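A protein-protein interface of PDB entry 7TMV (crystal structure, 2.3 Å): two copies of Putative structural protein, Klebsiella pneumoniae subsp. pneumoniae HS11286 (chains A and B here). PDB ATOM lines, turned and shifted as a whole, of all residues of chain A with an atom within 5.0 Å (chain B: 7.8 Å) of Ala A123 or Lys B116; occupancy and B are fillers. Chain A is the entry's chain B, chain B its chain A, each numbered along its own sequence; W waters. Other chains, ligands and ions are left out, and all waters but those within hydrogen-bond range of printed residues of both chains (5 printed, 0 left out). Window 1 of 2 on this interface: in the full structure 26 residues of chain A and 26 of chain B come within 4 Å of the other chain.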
ATOM      1  N   LEU A  21     -28.586   1.721  -8.116  1.00  0.00           N
ATOM      2  CA  LEU A  21     -28.199   2.698  -7.084  1.00  0.00           C
ATOM      3  C   LEU A  21     -28.215   4.117  -7.607  1.00  0.00           C
ATOM      4  O   LEU A  21     -28.523   5.069  -6.870  1.00  0.00           O
ATOM      5  CB  LEU A  21     -26.804   2.393  -6.530  1.00  0.00           C
ATOM      6  CG  LEU A  21     -26.804   1.155  -5.621  1.00  0.00           C
ATOM      7  CD1 LEU A  21     -25.410   0.877  -5.091  1.00  0.00           C
ATOM      8  CD2 LEU A  21     -27.777   1.328  -4.456  1.00  0.00           C
ATOM      9  N   ASP A  24     -31.772   5.186  -7.635  1.00  0.00           N
ATOM     10  CA  ASP A  24     -32.120   5.430  -6.235  1.00  0.00           C
ATOM     11  C   ASP A  24     -31.705   6.825  -5.821  1.00  0.00           C
ATOM     12  O   ASP A  24     -32.512   7.612  -5.284  1.00  0.00           O
ATOM     13  CB  ASP A  24     -31.396   4.380  -5.383  1.00  0.00           C
ATOM     14  CG  ASP A  24     -31.727   4.451  -3.901  1.00  0.00           C
ATOM     15  OD1 ASP A  24     -32.912   4.196  -3.549  1.00  0.00           O
ATOM     16  OD2 ASP A  24     -30.773   4.705  -3.092  1.00  0.00           O
ATOM     17  N   HIS A 119     -25.525  12.240   5.083  1.00  0.00           N
ATOM     18  CA  HIS A 119     -24.688  11.050   5.204  1.00  0.00           C
ATOM     19  C   HIS A 119     -25.281   9.879   4.457  1.00  0.00           C
ATOM     20  O   HIS A 119     -24.536   9.013   3.957  1.00  0.00           O
ATOM     21  CB  HIS A 119     -24.474  10.738   6.661  1.00  0.00           C
ATOM     22  CG  HIS A 119     -23.311  11.467   7.244  1.00  0.00           C
ATOM     23  ND1 HIS A 119     -22.016  11.032   7.102  1.00  0.00           N
ATOM     24  CD2 HIS A 119     -23.248  12.629   7.925  1.00  0.00           C
ATOM     25  CE1 HIS A 119     -21.203  11.877   7.710  1.00  0.00           C
ATOM     26  NE2 HIS A 119     -21.926  12.853   8.221  1.00  0.00           N
ATOM     27  N   TYR A 120     -26.601   9.836   4.312  1.00  0.00           N
ATOM     28  CA  TYR A 120     -27.129   8.897   3.330  1.00  0.00           C
ATOM     29  C   TYR A 120     -26.493   9.141   1.976  1.00  0.00           C
ATOM     30  O   TYR A 120     -26.093   8.198   1.280  1.00  0.00           O
ATOM     31  CB  TYR A 120     -28.640   9.027   3.200  1.00  0.00           C
ATOM     32  CG  TYR A 120     -29.260   7.949   2.330  1.00  0.00           C
ATOM     33  CD1 TYR A 120     -29.556   6.718   2.855  1.00  0.00           C
ATOM     34  CD2 TYR A 120     -29.554   8.186   0.998  1.00  0.00           C
ATOM     35  CE1 TYR A 120     -30.168   5.719   2.084  1.00  0.00           C
ATOM     36  CE2 TYR A 120     -30.147   7.231   0.215  1.00  0.00           C
ATOM     37  CZ  TYR A 120     -30.451   5.986   0.758  1.00  0.00           C
ATOM     38  OH  TYR A 120     -31.038   4.985  -0.001  1.00  0.00           O
ATOM     39  N   GLU A 121     -26.390  10.415   1.585  1.00  0.00           N
ATOM     40  CA  GLU A 121     -25.866  10.721   0.256  1.00  0.00           C
ATOM     41  C   GLU A 121     -24.376  10.427   0.163  1.00  0.00           C
ATOM     42  O   GLU A 121     -23.891   9.932  -0.869  1.00  0.00           O
ATOM     43  CB  GLU A 121     -26.135  12.170  -0.095  1.00  0.00           C
ATOM     44  CG  GLU A 121     -27.583  12.395  -0.365  1.00  0.00           C
ATOM     45  CD  GLU A 121     -27.859  13.800  -0.751  1.00  0.00           C
ATOM     46  OE1 GLU A 121     -27.713  14.661   0.143  1.00  0.00           O
ATOM     47  OE2 GLU A 121     -28.203  14.048  -1.931  1.00  0.00           O
ATOM     48  N   ILE A 122     -23.639  10.718   1.232  1.00  0.00           N
ATOM     49  CA  ILE A 122     -22.205  10.439   1.294  1.00  0.00           C
ATOM     50  C   ILE A 122     -21.948   8.951   1.063  1.00  0.00           C
ATOM     51  O   ILE A 122     -21.172   8.555   0.177  1.00  0.00           O
ATOM     52  CB  ILE A 122     -21.654  10.928   2.647  1.00  0.00           C
ATOM     53  CG1 ILE A 122     -21.785  12.444   2.677  1.00  0.00           C
ATOM     54  CG2 ILE A 122     -20.222  10.551   2.792  1.00  0.00           C
ATOM     55  CD1 ILE A 122     -21.388  13.182   4.001  1.00  0.00           C
ATOM     56  N   ALA A 123     -22.687   8.096   1.757  1.00  0.00           N
ATOM     57  CA  ALA A 123     -22.557   6.673   1.467  1.00  0.00           C
ATOM     58  C   ALA A 123     -22.875   6.356   0.004  1.00  0.00           C
ATOM     59  O   ALA A 123     -22.141   5.602  -0.666  1.00  0.00           O
ATOM     60  CB  ALA A 123     -23.491   5.870   2.380  1.00  0.00           C
ATOM     61  N   SER A 124     -24.006   6.880  -0.499  1.00  0.00           N
ATOM     62  CA  SER A 124     -24.467   6.482  -1.828  1.00  0.00           C
ATOM     63  C   SER A 124     -23.456   6.874  -2.893  1.00  0.00           C
ATOM     64  O   SER A 124     -23.126   6.084  -3.794  1.00  0.00           O
ATOM     65  CB  SER A 124     -25.811   7.143  -2.144  1.00  0.00           C
ATOM     66  OG  SER A 124     -26.783   6.760  -1.204  1.00  0.00           O
ATOM     67  N   TYR A 125     -22.983   8.118  -2.830  1.00  0.00           N
ATOM     68  CA  TYR A 125     -22.045   8.597  -3.838  1.00  0.00           C
ATOM     69  C   TYR A 125     -20.687   7.928  -3.701  1.00  0.00           C
ATOM     70  O   TYR A 125     -20.015   7.695  -4.720  1.00  0.00           O
ATOM     71  CB  TYR A 125     -21.918  10.101  -3.750  1.00  0.00           C
ATOM     72  CG  TYR A 125     -23.037  10.757  -4.508  1.00  0.00           C
ATOM     73  CD1 TYR A 125     -22.990  10.856  -5.881  1.00  0.00           C
ATOM     74  CD2 TYR A 125     -24.172  11.224  -3.861  1.00  0.00           C
ATOM     75  CE1 TYR A 125     -24.002  11.435  -6.580  1.00  0.00           C
ATOM     76  CE2 TYR A 125     -25.211  11.804  -4.567  1.00  0.00           C
ATOM     77  CZ  TYR A 125     -25.116  11.892  -5.928  1.00  0.00           C
ATOM     78  OH  TYR A 125     -26.114  12.463  -6.674  1.00  0.00           O
ATOM     79  N   GLY A 126     -20.271   7.559  -2.488  1.00  0.00           N
ATOM     80  CA  GLY A 126     -19.036   6.784  -2.386  1.00  0.00           C
ATOM     81  C   GLY A 126     -19.147   5.461  -3.128  1.00  0.00           C
ATOM     82  O   GLY A 126     -18.225   5.046  -3.853  1.00  0.00           O
ATOM     83  N   THR A 127     -20.289   4.787  -2.970  1.00  0.00           N
ATOM     84  CA  THR A 127     -20.473   3.515  -3.678  1.00  0.00           C
ATOM     85  C   THR A 127     -20.500   3.738  -5.175  1.00  0.00           C
ATOM     86  O   THR A 127     -19.951   2.934  -5.941  1.00  0.00           O
ATOM     87  CB  THR A 127     -21.767   2.840  -3.206  1.00  0.00           C
ATOM     88  OG1 THR A 127     -21.620   2.516  -1.815  1.00  0.00           O
ATOM     89  CG2 THR A 127     -22.076   1.543  -4.017  1.00  0.00           C
ATOM     90  N   MET B  86     -33.463   2.904  10.602  1.00  0.00           N
ATOM     91  CA  MET B  86     -32.535   1.779  10.583  1.00  0.00           C
ATOM     92  C   MET B  86     -33.253   0.520  10.138  1.00  0.00           C
ATOM     93  O   MET B  86     -32.687  -0.294   9.408  1.00  0.00           O
ATOM     94  CB  MET B  86     -31.876   1.585  11.956  1.00  0.00           C
ATOM     95  CG  MET B  86     -30.919   0.398  11.997  1.00  0.00           C
ATOM     96  SD  MET B  86     -29.480   0.528  10.886  1.00  0.00           S
ATOM     97  CE  MET B  86     -28.861   2.160  11.282  1.00  0.00           C
ATOM     98  N   LEU B  89     -33.195   0.496   6.519  1.00  0.00           N
ATOM     99  CA  LEU B  89     -31.890   0.207   5.891  1.00  0.00           C
ATOM    100  C   LEU B  89     -31.533  -1.279   6.003  1.00  0.00           C
ATOM    101  O   LEU B  89     -30.984  -1.890   5.063  1.00  0.00           O
ATOM    102  CB  LEU B  89     -30.792   1.082   6.513  1.00  0.00           C
ATOM    103  CG  LEU B  89     -31.008   2.593   6.315  1.00  0.00           C
ATOM    104  CD1 LEU B  89     -30.102   3.387   7.234  1.00  0.00           C
ATOM    105  CD2 LEU B  89     -30.785   3.033   4.885  1.00  0.00           C
ATOM    106  N   GLU B  92     -33.532  -3.266   3.496  1.00  0.00           N
ATOM    107  CA  GLU B  92     -32.971  -3.168   2.141  1.00  0.00           C
ATOM    108  C   GLU B  92     -31.740  -4.066   1.939  1.00  0.00           C
ATOM    109  O   GLU B  92     -31.578  -4.684   0.876  1.00  0.00           O
ATOM    110  CB  GLU B  92     -32.627  -1.718   1.837  1.00  0.00           C
ATOM    111  CG  GLU B  92     -33.856  -0.855   1.803  1.00  0.00           C
ATOM    112  CD  GLU B  92     -33.782   0.297   0.812  1.00  0.00           C
ATOM    113  OE1 GLU B  92     -33.738   0.011  -0.416  1.00  0.00           O
ATOM    114  OE2 GLU B  92     -33.813   1.470   1.267  1.00  0.00           O
ATOM    115  N   ALA B 109     -23.574  -5.059  -3.680  1.00  0.00           N
ATOM    116  CA  ALA B 109     -24.778  -4.361  -3.210  1.00  0.00           C
ATOM    117  C   ALA B 109     -24.933  -4.420  -1.701  1.00  0.00           C
ATOM    118  O   ALA B 109     -25.469  -3.484  -1.078  1.00  0.00           O
ATOM    119  CB  ALA B 109     -26.025  -4.957  -3.863  1.00  0.00           C
ATOM    120  N   LEU B 110     -24.471  -5.509  -1.096  1.00  0.00           N
ATOM    121  CA  LEU B 110     -24.539  -5.666   0.343  1.00  0.00           C
ATOM    122  C   LEU B 110     -23.575  -4.717   1.028  1.00  0.00           C
ATOM    123  O   LEU B 110     -23.941  -4.067   2.014  1.00  0.00           O
ATOM    124  CB  LEU B 110     -24.216  -7.118   0.691  1.00  0.00           C
ATOM    125  CG  LEU B 110     -24.924  -7.781   1.864  1.00  0.00           C
ATOM    126  CD1 LEU B 110     -26.416  -7.701   1.693  1.00  0.00           C
ATOM    127  CD2 LEU B 110     -24.441  -9.202   1.967  1.00  0.00           C
ATOM    128  N   ILE B 111     -22.367  -4.557   0.487  1.00  0.00           N
ATOM    129  CA  ILE B 111     -21.463  -3.559   1.044  1.00  0.00           C
ATOM    130  C   ILE B 111     -22.099  -2.178   0.969  1.00  0.00           C
ATOM    131  O   ILE B 111     -21.991  -1.374   1.912  1.00  0.00           O
ATOM    132  CB  ILE B 111     -20.102  -3.576   0.333  1.00  0.00           C
ATOM    133  CG1 ILE B 111     -19.287  -4.790   0.749  1.00  0.00           C
ATOM    134  CG2 ILE B 111     -19.311  -2.288   0.693  1.00  0.00           C
ATOM    135  CD1 ILE B 111     -18.341  -5.240  -0.373  1.00  0.00           C
ATOM    136  N   ALA B 112     -22.741  -1.864  -0.162  1.00  0.00           N
ATOM    137  CA  ALA B 112     -23.378  -0.554  -0.297  1.00  0.00           C
ATOM    138  C   ALA B 112     -24.395  -0.341   0.811  1.00  0.00           C
ATOM    139  O   ALA B 112     -24.432   0.722   1.459  1.00  0.00           O
ATOM    140  CB  ALA B 112     -24.050  -0.441  -1.678  1.00  0.00           C
ATOM    141  N   ALA B 113     -25.249  -1.351   1.036  1.00  0.00           N
ATOM    142  CA  ALA B 113     -26.300  -1.222   2.044  1.00  0.00           C
ATOM    143  C   ALA B 113     -25.688  -1.072   3.423  1.00  0.00           C
ATOM    144  O   ALA B 113     -26.169  -0.285   4.258  1.00  0.00           O
ATOM    145  CB  ALA B 113     -27.239  -2.429   1.985  1.00  0.00           C
ATOM    146  N   ALA B 114     -24.604  -1.803   3.681  1.00  0.00           N
ATOM    147  CA  ALA B 114     -23.957  -1.681   4.983  1.00  0.00           C
ATOM    148  C   ALA B 114     -23.329  -0.305   5.179  1.00  0.00           C
ATOM    149  O   ALA B 114     -23.285   0.218   6.317  1.00  0.00           O
ATOM    150  CB  ALA B 114     -22.928  -2.797   5.143  1.00  0.00           C
ATOM    151  N   GLN B 115     -22.822   0.305   4.102  1.00  0.00           N
ATOM    152  CA  GLN B 115     -22.271   1.663   4.248  1.00  0.00           C
ATOM    153  C   GLN B 115     -23.374   2.673   4.523  1.00  0.00           C
ATOM    154  O   GLN B 115     -23.167   3.637   5.286  1.00  0.00           O
ATOM    155  CB  GLN B 115     -21.451   2.028   3.018  1.00  0.00           C
ATOM    156  CG  GLN B 115     -20.127   1.222   3.007  1.00  0.00           C
ATOM    157  CD  GLN B 115     -19.173   1.632   1.920  1.00  0.00           C
ATOM    158  OE1 GLN B 115     -18.087   2.195   2.198  1.00  0.00           O
ATOM    159  NE2 GLN B 115     -19.534   1.334   0.677  1.00  0.00           N
ATOM    160  N   LYS B 116     -24.556   2.468   3.931  1.00  0.00           N
ATOM    161  CA  LYS B 116     -25.687   3.329   4.287  1.00  0.00           C
ATOM    162  C   LYS B 116     -26.030   3.202   5.777  1.00  0.00           C
ATOM    163  O   LYS B 116     -26.217   4.214   6.460  1.00  0.00           O
ATOM    164  CB  LYS B 116     -26.903   2.992   3.420  1.00  0.00           C
ATOM    165  CG  LYS B 116     -26.821   3.519   1.972  1.00  0.00           C
ATOM    166  CD  LYS B 116     -27.992   3.006   1.182  1.00  0.00           C
ATOM    167  CE  LYS B 116     -27.849   3.166  -0.324  1.00  0.00           C
ATOM    168  NZ  LYS B 116     -26.894   4.183  -0.639  1.00  0.00           N
ATOM    169  N   VAL B 117     -26.052   1.971   6.315  1.00  0.00           N
ATOM    170  CA  VAL B 117     -26.276   1.807   7.762  1.00  0.00           C
ATOM    171  C   VAL B 117     -25.209   2.553   8.567  1.00  0.00           C
ATOM    172  O   VAL B 117     -25.505   3.338   9.496  1.00  0.00           O
ATOM    173  CB  VAL B 117     -26.304   0.301   8.111  1.00  0.00           C
ATOM    174  CG1 VAL B 117     -25.995   0.065   9.609  1.00  0.00           C
ATOM    175  CG2 VAL B 117     -27.642  -0.320   7.709  1.00  0.00           C
ATOM    176  N   GLU B 118     -23.942   2.317   8.236  1.00  0.00           N
ATOM    177  CA  GLU B 118     -22.866   2.937   8.979  1.00  0.00           C
ATOM    178  C   GLU B 118     -22.980   4.456   8.947  1.00  0.00           C
ATOM    179  O   GLU B 118     -22.737   5.130   9.958  1.00  0.00           O
ATOM    180  CB  GLU B 118     -21.513   2.500   8.398  1.00  0.00           C
ATOM    181  CG  GLU B 118     -21.142   1.053   8.629  1.00  0.00           C
ATOM    182  CD  GLU B 118     -21.527   0.621  10.031  1.00  0.00           C
ATOM    183  OE1 GLU B 118     -21.206   1.448  10.940  1.00  0.00           O
ATOM    184  OE2 GLU B 118     -22.170  -0.477  10.192  1.00  0.00           O
ATOM    185  N   HIS B 119     -23.346   5.029   7.804  1.00  0.00           N
ATOM    186  CA  HIS B 119     -23.374   6.495   7.755  1.00  0.00           C
ATOM    187  C   HIS B 119     -24.588   7.076   8.473  1.00  0.00           C
ATOM    188  O   HIS B 119     -24.493   8.179   9.044  1.00  0.00           O
ATOM    189  CB  HIS B 119     -23.288   6.976   6.304  1.00  0.00           C
ATOM    190  CG  HIS B 119     -21.874   7.134   5.828  1.00  0.00           C
ATOM    191  ND1 HIS B 119     -21.128   8.267   6.065  1.00  0.00           N
ATOM    192  CD2 HIS B 119     -21.062   6.285   5.157  1.00  0.00           C
ATOM    193  CE1 HIS B 119     -19.927   8.121   5.534  1.00  0.00           C
ATOM    194  NE2 HIS B 119     -19.857   6.918   4.993  1.00  0.00           N
ATOM    195  N   TYR B 120     -25.715   6.358   8.515  1.00  0.00           N
ATOM    196  CA  TYR B 120     -26.765   6.782   9.448  1.00  0.00           C
ATOM    197  C   TYR B 120     -26.174   6.934  10.854  1.00  0.00           C
ATOM    198  O   TYR B 120     -26.437   7.917  11.571  1.00  0.00           O
ATOM    199  CB  TYR B 120     -27.923   5.777   9.460  1.00  0.00           C
ATOM    200  CG  TYR B 120     -29.112   6.232  10.291  1.00  0.00           C
ATOM    201  CD1 TYR B 120     -30.091   7.075   9.748  1.00  0.00           C
ATOM    202  CD2 TYR B 120     -29.276   5.801  11.612  1.00  0.00           C
ATOM    203  CE1 TYR B 120     -31.207   7.500  10.514  1.00  0.00           C
ATOM    204  CE2 TYR B 120     -30.376   6.231  12.381  1.00  0.00           C
ATOM    205  CZ  TYR B 120     -31.329   7.077  11.823  1.00  0.00           C
ATOM    206  OH  TYR B 120     -32.415   7.499  12.558  1.00  0.00           O
ATOM    207  N   GLU B 121     -25.339   5.967  11.250  1.00  0.00           N
ATOM    208  CA  GLU B 121     -24.794   5.999  12.607  1.00  0.00           C
ATOM    209  C   GLU B 121     -23.728   7.075  12.782  1.00  0.00           C
ATOM    210  O   GLU B 121     -23.607   7.658  13.868  1.00  0.00           O
ATOM    211  CB  GLU B 121     -24.226   4.648  12.944  1.00  0.00           C
ATOM    212  CG  GLU B 121     -25.274   3.617  13.022  1.00  0.00           C
ATOM    213  CD  GLU B 121     -24.703   2.335  13.518  1.00  0.00           C
ATOM    214  OE1 GLU B 121     -23.869   1.758  12.785  1.00  0.00           O
ATOM    215  OE2 GLU B 121     -25.106   1.918  14.632  1.00  0.00           O
ATOM    216  N   ILE B 122     -22.895   7.295  11.761  1.00  0.00           N
ATOM    217  CA  ILE B 122     -21.881   8.349  11.826  1.00  0.00           C
ATOM    218  C   ILE B 122     -22.559   9.695  12.081  1.00  0.00           C
ATOM    219  O   ILE B 122     -22.193  10.442  13.002  1.00  0.00           O
ATOM    220  CB  ILE B 122     -21.043   8.354  10.529  1.00  0.00           C
ATOM    221  CG1 ILE B 122     -20.049   7.171  10.555  1.00  0.00           C
ATOM    222  CG2 ILE B 122     -20.366   9.718  10.322  1.00  0.00           C
ATOM    223  CD1 ILE B 122     -19.394   6.808   9.202  1.00  0.00           C
ATOM    224  N   ASP B 155     -16.716   2.103   8.294  1.00  0.00           N
ATOM    225  CA  ASP B 155     -17.033   2.568   6.945  1.00  0.00           C
ATOM    226  C   ASP B 155     -15.817   2.491   6.028  1.00  0.00           C
ATOM    227  O   ASP B 155     -15.926   2.039   4.882  1.00  0.00           O
ATOM    228  CB  ASP B 155     -17.586   3.987   6.969  1.00  0.00           C
ATOM    229  CG  ASP B 155     -17.882   4.488   5.581  1.00  0.00           C
ATOM    230  OD1 ASP B 155     -18.492   3.714   4.799  1.00  0.00           O
ATOM    231  OD2 ASP B 155     -17.454   5.601   5.242  1.00  0.00           O
ATOM    232  N   LEU B 158     -15.215  -1.022   4.944  1.00  0.00           N
ATOM    233  CA  LEU B 158     -16.171  -1.427   3.911  1.00  0.00           C
ATOM    234  C   LEU B 158     -15.784  -0.858   2.552  1.00  0.00           C
ATOM    235  O   LEU B 158     -15.893  -1.552   1.542  1.00  0.00           O
ATOM    236  CB  LEU B 158     -17.599  -1.005   4.287  1.00  0.00           C
ATOM    237  CG  LEU B 158     -18.192  -1.874   5.423  1.00  0.00           C
ATOM    238  CD1 LEU B 158     -19.443  -1.268   5.983  1.00  0.00           C
ATOM    239  CD2 LEU B 158     -18.451  -3.321   4.993  1.00  0.00           C
ATOM    240  N   THR B 159     -15.289   0.381   2.501  1.00  0.00           N
ATOM    241  CA  THR B 159     -14.869   0.922   1.208  1.00  0.00           C
ATOM    242  C   THR B 159     -13.725   0.089   0.638  1.00  0.00           C
ATOM    243  O   THR B 159     -13.688  -0.203  -0.572  1.00  0.00           O
ATOM    244  CB  THR B 159     -14.448   2.395   1.326  1.00  0.00           C
ATOM    245  OG1 THR B 159     -15.509   3.199   1.859  1.00  0.00           O
ATOM    246  CG2 THR B 159     -14.103   2.959  -0.065  1.00  0.00           C
HETATM  247  O   HOH W   1     -23.722   3.093   0.213  1.00  0.00           O
HETATM  248  O   HOH W   2     -20.208   4.145   0.507  1.00  0.00           O
HETATM  249  O   HOH W   3     -17.375   2.692  -1.551  1.00  0.00           O
HETATM  250  O   HOH W   4     -28.410   5.032  -3.604  1.00  0.00           O
HETATM  251  O   HOH W   5     -34.216   3.293  -1.079  1.00  0.00           O
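OG1 of Thr A127 lies within hydrogen-bond range of NE2 of Gln B115, at 3.5 Å.
A ring nitrogen (ND1) of His B119 sits at hydrogen-bond distance from a ring nitrogen (ND1) of His A119 (3.1 Å).
The side-chain amino group (NZ) of Lys B116 lies within hydrogen-bond range of the side-chain hydroxyl (OG) of Ser A124, at 2.6 Å.
OG1 of Thr A127 lies within hydrogen-bond range of O of Ala A123, 3.3 Å away.
OE1 of Gln B115 sits close to OD1 of Asp B155 (3.0 Å).
A ring nitrogen (NE2) of His B119 is in hydrogen-bond range of the side-chain carboxylate (OD2) of Asp B155.
The side-chain carboxylate (OD2) of Asp A24 lies within hydrogen-bond range of the side-chain hydroxyl (OH) of Tyr A120 (3.1 Å).
O of Tyr A120 lies within hydrogen-bond range of OG of Ser A124.
OE1 of Gln B115 is in hydrogen-bond range of OG1 of Thr B159.
Among the printed residues, pairs that only touch across the chains: His A119 with Ile B122 (3.5 Å), Tyr A120 with Lys B116 (3.6 Å), Thr A127 with Ala B112 (3.6 Å), Ile A122 with His B119 (3.7 Å), Ala A123 with Gln B115 (3.7 Å), Ala A123 with His B119 (3.7 Å), Ala A123 with Lys B116 (3.9 Å), Leu A21 with Ala B112 (3.9 Å) and Tyr A120 with Leu B89 (3.9 Å).
Ala A123 touches three residues of chain B.
Lys B116 touches three residues of chain A.
Printed residues of chain A within 4 Å of His B119: His A119 (3.1 Å), Ile A122 (3.7 Å) and Ala A123 (3.7 Å).
Of the printed residues of chain A, Leu B89 touches Tyr A120 (3.9 Å).
Ala B109 touches none of the printed residues of chain A.
Ala B113 touches none of the printed residues of chain A.
The nearest residue of chain A that does not touch Lys B116 is Asp A24 (4.3 Å).
The nearest printed residue of chain B that does not touch Ile A122 is Asp B155 (6.2 Å).
Printed residues of chain A that touch a printed residue of chain B: Leu A21, His A119, Tyr A120, Ile A122, Ala A123, Ser A124 and Thr A127.
Hydrophobic or aromatic side chains of chain A that line the printed part of chain B: Leu A21, His A119, Tyr A120, Ile A122 and Ala A123.
Along chain A the printed residues that touch a printed residue of chain B span positions 21 to 127.
Printed residues of chain B that touch a printed residue of chain A: Leu B89, Ala B112, Gln B115, Lys B116, His B119 and Ile B122.
Among the printed residues, 12 pairs touch across the chains.
Among the printed residues, no Asp or Glu carboxylate lies within 4 Å of a Lys or Arg side-chain nitrogen of the other chain.
His A119 touches its own counterpart, His B119.
His A119 touches Ile B122, and with the chains exchanged Ile A122 touches His B119.
Positions printed for both chains: 119, 120, 121 and 122.
Of the 12 pairs that touch across the chains among the printed residues, 3 have their exchanged pair printed and touching as well.
Water W4 lies within hydrogen-bond range of OD2 of Asp A24 (2.4 Å), O of Leu A21 (3.3 Å), OG of Ser A124 (3.4 Å) and NZ of Lys B116 (3.4 Å).
Water W2 lies within hydrogen-bond range of the backbone carbonyl oxygen (O) of Ala A123 (2.7 Å), the side-chain amide nitrogen (NE2) of Gln B115 (2.9 Å) and the side-chain hydroxyl (OG1) of Thr A127 (3.2 Å).
Water W1 lies within hydrogen-bond range of O of Ala B112, OG1 of Thr A127, O of Ala A123 and NZ of Lys B116.
Water W5 bridges OD1 of Asp A24 (2.9 Å) and OE2 of Glu B92 (3.0 Å).
Water W3 lies within hydrogen-bond range of NE2 of Gln B115 (3.4 Å) and O of Gly A126 (3.4 Å).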
